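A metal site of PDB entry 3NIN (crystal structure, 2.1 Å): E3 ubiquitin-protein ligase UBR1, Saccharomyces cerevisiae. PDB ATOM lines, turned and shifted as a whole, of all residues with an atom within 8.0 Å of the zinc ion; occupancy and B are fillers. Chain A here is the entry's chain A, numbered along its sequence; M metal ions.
The side-chain sulfur of Cys 24 sits close to the backbone NH of Glu 26, 3.6 Å away.
Merely in contact with the zinc ion: Asp 44.
Of the 21 residues printed, 5 come within 4 Å of the zinc ion.
The nearest printed residue that does not touch the zinc ion is Glu 26 (4.4 Å).
The zinc ion is bound by ND1 of His 45 (2.0 Å), SG of Cys 24 (2.1 Å), ND1 of His 48 (2.2 Å) and SG of Cys 27 (2.6 Å).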
ATOM      1  N   ARG A  23      -9.165  14.922  19.604  1.00  0.00           N
ATOM      2  CA  ARG A  23      -9.678  15.073  20.951  1.00  0.00           C
ATOM      3  C   ARG A  23     -11.021  15.777  20.879  1.00  0.00           C
ATOM      4  O   ARG A  23     -11.229  16.627  20.024  1.00  0.00           O
ATOM      5  CB  ARG A  23      -8.730  15.888  21.834  1.00  0.00           C
ATOM      6  CG  ARG A  23      -7.431  15.198  22.186  1.00  0.00           C
ATOM      7  CD  ARG A  23      -6.550  16.159  22.982  1.00  0.00           C
ATOM      8  NE  ARG A  23      -5.271  15.556  23.344  1.00  0.00           N
ATOM      9  CZ  ARG A  23      -4.122  15.801  22.710  1.00  0.00           C
ATOM     10  NH1 ARG A  23      -4.075  16.638  21.685  1.00  0.00           N
ATOM     11  NH2 ARG A  23      -3.012  15.213  23.130  1.00  0.00           N
ATOM     12  N   CYS A  24     -11.920  15.422  21.795  1.00  0.00           N
ATOM     13  CA  CYS A  24     -13.207  16.104  21.928  1.00  0.00           C
ATOM     14  C   CYS A  24     -13.326  16.577  23.380  1.00  0.00           C
ATOM     15  O   CYS A  24     -13.155  15.773  24.300  1.00  0.00           O
ATOM     16  CB  CYS A  24     -14.363  15.172  21.563  1.00  0.00           C
ATOM     17  SG  CYS A  24     -16.010  15.852  21.815  1.00  0.00           S
ATOM     18  N   HIS A  25     -13.616  17.865  23.565  1.00  0.00           N
ATOM     19  CA  HIS A  25     -13.735  18.433  24.908  1.00  0.00           C
ATOM     20  C   HIS A  25     -14.912  17.819  25.651  1.00  0.00           C
ATOM     21  O   HIS A  25     -14.793  17.479  26.838  1.00  0.00           O
ATOM     22  CB  HIS A  25     -13.850  19.960  24.858  1.00  0.00           C
ATOM     23  CG  HIS A  25     -14.147  20.579  26.188  1.00  0.00           C
ATOM     24  ND1 HIS A  25     -13.276  20.500  27.263  1.00  0.00           N
ATOM     25  CD2 HIS A  25     -15.216  21.293  26.621  1.00  0.00           C
ATOM     26  CE1 HIS A  25     -13.810  21.137  28.297  1.00  0.00           C
ATOM     27  NE2 HIS A  25     -14.981  21.622  27.937  1.00  0.00           N
ATOM     28  N   GLU A  26     -16.028  17.666  24.956  1.00  0.00           N
ATOM     29  CA  GLU A  26     -17.242  17.073  25.528  1.00  0.00           C
ATOM     30  C   GLU A  26     -17.100  15.574  25.854  1.00  0.00           C
ATOM     31  O   GLU A  26     -17.527  15.119  26.916  1.00  0.00           O
ATOM     32  CB  GLU A  26     -18.448  17.296  24.601  1.00  0.00           C
ATOM     33  CG  GLU A  26     -18.967  18.737  24.559  1.00  0.00           C
ATOM     34  CD  GLU A  26     -18.142  19.672  23.677  1.00  0.00           C
ATOM     35  OE1 GLU A  26     -17.102  19.227  23.113  1.00  0.00           O
ATOM     36  OE2 GLU A  26     -18.518  20.849  23.550  1.00  0.00           O
ATOM     37  N   CYS A  27     -16.493  14.827  24.930  1.00  0.00           N
ATOM     38  CA  CYS A  27     -16.522  13.359  25.012  1.00  0.00           C
ATOM     39  C   CYS A  27     -15.395  12.729  25.830  1.00  0.00           C
ATOM     40  O   CYS A  27     -15.614  11.693  26.467  1.00  0.00           O
ATOM     41  CB  CYS A  27     -16.589  12.750  23.605  1.00  0.00           C
ATOM     42  SG  CYS A  27     -18.233  12.814  22.854  1.00  0.00           S
ATOM     43  N   GLY A  28     -14.214  13.331  25.831  1.00  0.00           N
ATOM     44  CA  GLY A  28     -13.065  12.802  26.565  1.00  0.00           C
ATOM     45  C   GLY A  28     -13.143  13.021  28.058  1.00  0.00           C
ATOM     46  O   GLY A  28     -13.530  14.103  28.510  1.00  0.00           O
ATOM     47  N   LEU A  35      -8.425   9.785  19.694  1.00  0.00           N
ATOM     48  CA  LEU A  35      -8.952   8.904  18.634  1.00  0.00           C
ATOM     49  C   LEU A  35      -8.085   8.998  17.379  1.00  0.00           C
ATOM     50  O   LEU A  35      -7.709  10.096  16.976  1.00  0.00           O
ATOM     51  CB  LEU A  35     -10.384   9.332  18.272  1.00  0.00           C
ATOM     52  CG  LEU A  35     -11.501   9.115  19.292  1.00  0.00           C
ATOM     53  CD1 LEU A  35     -12.791   9.771  18.843  1.00  0.00           C
ATOM     54  CD2 LEU A  35     -11.715   7.631  19.545  1.00  0.00           C
ATOM     55  N   PHE A  40     -12.308   8.097  14.473  1.00  0.00           N
ATOM     56  CA  PHE A  40     -13.075   9.327  14.723  1.00  0.00           C
ATOM     57  C   PHE A  40     -14.276   9.438  13.768  1.00  0.00           C
ATOM     58  O   PHE A  40     -14.107   9.487  12.544  1.00  0.00           O
ATOM     59  CB  PHE A  40     -12.193  10.580  14.640  1.00  0.00           C
ATOM     60  CG  PHE A  40     -12.957  11.875  14.763  1.00  0.00           C
ATOM     61  CD1 PHE A  40     -13.216  12.433  16.019  1.00  0.00           C
ATOM     62  CD2 PHE A  40     -13.414  12.552  13.633  1.00  0.00           C
ATOM     63  CE1 PHE A  40     -13.913  13.632  16.150  1.00  0.00           C
ATOM     64  CE2 PHE A  40     -14.134  13.759  13.749  1.00  0.00           C
ATOM     65  CZ  PHE A  40     -14.377  14.290  15.007  1.00  0.00           C
ATOM     66  N   ASN A  41     -15.471   9.494  14.340  1.00  0.00           N
ATOM     67  CA  ASN A  41     -16.685   9.651  13.572  1.00  0.00           C
ATOM     68  C   ASN A  41     -17.297  11.024  13.827  1.00  0.00           C
ATOM     69  O   ASN A  41     -17.701  11.316  14.959  1.00  0.00           O
ATOM     70  CB  ASN A  41     -17.683   8.533  13.907  1.00  0.00           C
ATOM     71  CG  ASN A  41     -18.868   8.469  12.928  1.00  0.00           C
ATOM     72  OD1 ASN A  41     -19.137   9.400  12.166  1.00  0.00           O
ATOM     73  ND2 ASN A  41     -19.584   7.343  12.966  1.00  0.00           N
ATOM     74  N   PRO A  42     -17.352  11.886  12.793  1.00  0.00           N
ATOM     75  CA  PRO A  42     -17.950  13.224  12.918  1.00  0.00           C
ATOM     76  C   PRO A  42     -19.375  13.205  13.499  1.00  0.00           C
ATOM     77  O   PRO A  42     -19.745  14.110  14.239  1.00  0.00           O
ATOM     78  CB  PRO A  42     -17.987  13.724  11.473  1.00  0.00           C
ATOM     79  CG  PRO A  42     -16.844  13.042  10.819  1.00  0.00           C
ATOM     80  CD  PRO A  42     -16.768  11.674  11.453  1.00  0.00           C
ATOM     81  N   LYS A  43     -20.136  12.158  13.174  1.00  0.00           N
ATOM     82  CA  LYS A  43     -21.515  12.013  13.623  1.00  0.00           C
ATOM     83  C   LYS A  43     -21.664  11.815  15.145  1.00  0.00           C
ATOM     84  O   LYS A  43     -22.775  11.853  15.676  1.00  0.00           O
ATOM     85  CB  LYS A  43     -22.204  10.870  12.869  1.00  0.00           C
ATOM     86  CG  LYS A  43     -22.511  11.189  11.411  1.00  0.00           C
ATOM     87  CD  LYS A  43     -22.434   9.931  10.562  1.00  0.00           C
ATOM     88  CE  LYS A  43     -22.449  10.276   9.082  1.00  0.00           C
ATOM     89  NZ  LYS A  43     -21.921   9.131   8.275  1.00  0.00           N
ATOM     90  N   ASP A  44     -20.538  11.601  15.829  1.00  0.00           N
ATOM     91  CA  ASP A  44     -20.507  11.482  17.286  1.00  0.00           C
ATOM     92  C   ASP A  44     -20.294  12.835  17.970  1.00  0.00           C
ATOM     93  O   ASP A  44     -20.518  12.975  19.178  1.00  0.00           O
ATOM     94  CB  ASP A  44     -19.400  10.522  17.724  1.00  0.00           C
ATOM     95  CG  ASP A  44     -19.799   9.056  17.631  1.00  0.00           C
ATOM     96  OD1 ASP A  44     -21.004   8.747  17.726  1.00  0.00           O
ATOM     97  OD2 ASP A  44     -18.886   8.213  17.487  1.00  0.00           O
ATOM     98  N   HIS A  45     -19.856  13.836  17.203  1.00  0.00           N
ATOM     99  CA  HIS A  45     -19.381  15.095  17.769  1.00  0.00           C
ATOM    100  C   HIS A  45     -19.900  16.308  17.009  1.00  0.00           C
ATOM    101  O   HIS A  45     -19.139  17.245  16.742  1.00  0.00           O
ATOM    102  CB  HIS A  45     -17.849  15.122  17.792  1.00  0.00           C
ATOM    103  CG  HIS A  45     -17.236  13.843  18.263  1.00  0.00           C
ATOM    104  ND1 HIS A  45     -17.155  13.514  19.603  1.00  0.00           N
ATOM    105  CD2 HIS A  45     -16.712  12.804  17.581  1.00  0.00           C
ATOM    106  CE1 HIS A  45     -16.589  12.328  19.721  1.00  0.00           C
ATOM    107  NE2 HIS A  45     -16.305  11.879  18.512  1.00  0.00           N
ATOM    108  N   VAL A  46     -21.186  16.293  16.687  1.00  0.00           N
ATOM    109  CA  VAL A  46     -21.805  17.305  15.811  1.00  0.00           C
ATOM    110  C   VAL A  46     -21.601  18.754  16.284  1.00  0.00           C
ATOM    111  O   VAL A  46     -21.113  19.605  15.523  1.00  0.00           O
ATOM    112  CB  VAL A  46     -23.292  16.982  15.515  1.00  0.00           C
ATOM    113  CG1 VAL A  46     -24.049  18.201  14.949  1.00  0.00           C
ATOM    114  CG2 VAL A  46     -23.391  15.794  14.556  1.00  0.00           C
ATOM    115  N   ASN A  47     -21.983  19.040  17.526  1.00  0.00           N
ATOM    116  CA  ASN A  47     -21.800  20.396  18.047  1.00  0.00           C
ATOM    117  C   ASN A  47     -20.779  20.437  19.188  1.00  0.00           C
ATOM    118  O   ASN A  47     -20.875  21.266  20.100  1.00  0.00           O
ATOM    119  CB  ASN A  47     -23.140  21.052  18.426  1.00  0.00           C
ATOM    120  CG  ASN A  47     -23.748  21.868  17.276  1.00  0.00           C
ATOM    121  OD1 ASN A  47     -23.606  21.522  16.093  1.00  0.00           O
ATOM    122  ND2 ASN A  47     -24.433  22.962  17.621  1.00  0.00           N
ATOM    123  N   HIS A  48     -19.810  19.535  19.101  1.00  0.00           N
ATOM    124  CA  HIS A  48     -18.752  19.423  20.108  1.00  0.00           C
ATOM    125  C   HIS A  48     -17.516  20.250  19.729  1.00  0.00           C
ATOM    126  O   HIS A  48     -17.410  20.753  18.612  1.00  0.00           O
ATOM    127  CB  HIS A  48     -18.397  17.956  20.361  1.00  0.00           C
ATOM    128  CG  HIS A  48     -19.535  17.146  20.919  1.00  0.00           C
ATOM    129  ND1 HIS A  48     -19.471  15.772  21.057  1.00  0.00           N
ATOM    130  CD2 HIS A  48     -20.759  17.508  21.367  1.00  0.00           C
ATOM    131  CE1 HIS A  48     -20.607  15.336  21.573  1.00  0.00           C
ATOM    132  NE2 HIS A  48     -21.403  16.370  21.762  1.00  0.00           N
ATOM    133  N   HIS A  49     -16.615  20.414  20.692  1.00  0.00           N
ATOM    134  CA  HIS A  49     -15.359  21.130  20.473  1.00  0.00           C
ATOM    135  C   HIS A  49     -14.243  20.114  20.245  1.00  0.00           C
ATOM    136  O   HIS A  49     -13.708  19.533  21.195  1.00  0.00           O
ATOM    137  CB  HIS A  49     -15.046  22.043  21.656  1.00  0.00           C
ATOM    138  CG  HIS A  49     -16.049  23.152  21.834  1.00  0.00           C
ATOM    139  ND1 HIS A  49     -17.313  22.945  22.329  1.00  0.00           N
ATOM    140  CD2 HIS A  49     -15.953  24.474  21.578  1.00  0.00           C
ATOM    141  CE1 HIS A  49     -17.957  24.094  22.371  1.00  0.00           C
ATOM    142  NE2 HIS A  49     -17.157  25.044  21.924  1.00  0.00           N
ATOM    143  N   VAL A  50     -13.912  19.898  18.972  1.00  0.00           N
ATOM    144  CA  VAL A  50     -12.935  18.892  18.559  1.00  0.00           C
ATOM    145  C   VAL A  50     -11.663  19.579  18.081  1.00  0.00           C
ATOM    146  O   VAL A  50     -11.727  20.563  17.333  1.00  0.00           O
ATOM    147  CB  VAL A  50     -13.510  17.986  17.425  1.00  0.00           C
ATOM    148  CG1 VAL A  50     -12.454  16.998  16.893  1.00  0.00           C
ATOM    149  CG2 VAL A  50     -14.735  17.238  17.906  1.00  0.00           C
ATOM    150  N   TRP A  71     -14.275   7.760  27.698  1.00  0.00           N
ATOM    151  CA  TRP A  71     -15.325   8.599  27.099  1.00  0.00           C
ATOM    152  C   TRP A  71     -16.569   8.766  27.969  1.00  0.00           C
ATOM    153  O   TRP A  71     -17.091   7.795  28.523  1.00  0.00           O
ATOM    154  CB  TRP A  71     -15.705   8.052  25.724  1.00  0.00           C
ATOM    155  CG  TRP A  71     -14.497   7.790  24.882  1.00  0.00           C
ATOM    156  CD1 TRP A  71     -13.970   6.573  24.585  1.00  0.00           C
ATOM    157  CD2 TRP A  71     -13.648   8.763  24.271  1.00  0.00           C
ATOM    158  NE1 TRP A  71     -12.844   6.729  23.808  1.00  0.00           N
ATOM    159  CE2 TRP A  71     -12.627   8.062  23.602  1.00  0.00           C
ATOM    160  CE3 TRP A  71     -13.665  10.163  24.207  1.00  0.00           C
ATOM    161  CZ2 TRP A  71     -11.622   8.707  22.878  1.00  0.00           C
ATOM    162  CZ3 TRP A  71     -12.664  10.809  23.491  1.00  0.00           C
ATOM    163  CH2 TRP A  71     -11.654  10.074  22.832  1.00  0.00           C
ATOM    164  N   SER A  73     -19.438   9.602  26.829  1.00  0.00           N
ATOM    165  CA  SER A  73     -20.556   9.158  26.009  1.00  0.00           C
ATOM    166  C   SER A  73     -20.125   7.989  25.121  1.00  0.00           C
ATOM    167  O   SER A  73     -18.963   7.943  24.694  1.00  0.00           O
ATOM    168  CB  SER A  73     -21.071  10.322  25.152  1.00  0.00           C
ATOM    169  OG  SER A  73     -21.894   9.864  24.092  1.00  0.00           O
ATOM    170  N   LEU A  75     -19.333   5.809  21.940  1.00  0.00           N
ATOM    171  CA  LEU A  75     -18.833   6.189  20.614  1.00  0.00           C
ATOM    172  C   LEU A  75     -19.334   5.217  19.559  1.00  0.00           C
ATOM    173  O   LEU A  75     -19.646   4.067  19.855  1.00  0.00           O
ATOM    174  CB  LEU A  75     -17.303   6.233  20.597  1.00  0.00           C
ATOM    175  CG  LEU A  75     -16.612   7.384  21.339  1.00  0.00           C
ATOM    176  CD1 LEU A  75     -15.108   7.311  21.168  1.00  0.00           C
ATOM    177  CD2 LEU A  75     -17.142   8.747  20.883  1.00  0.00           C
HETATM  178 ZN    ZN M   1     -17.558  14.646  21.147  1.00  0.00          ZN
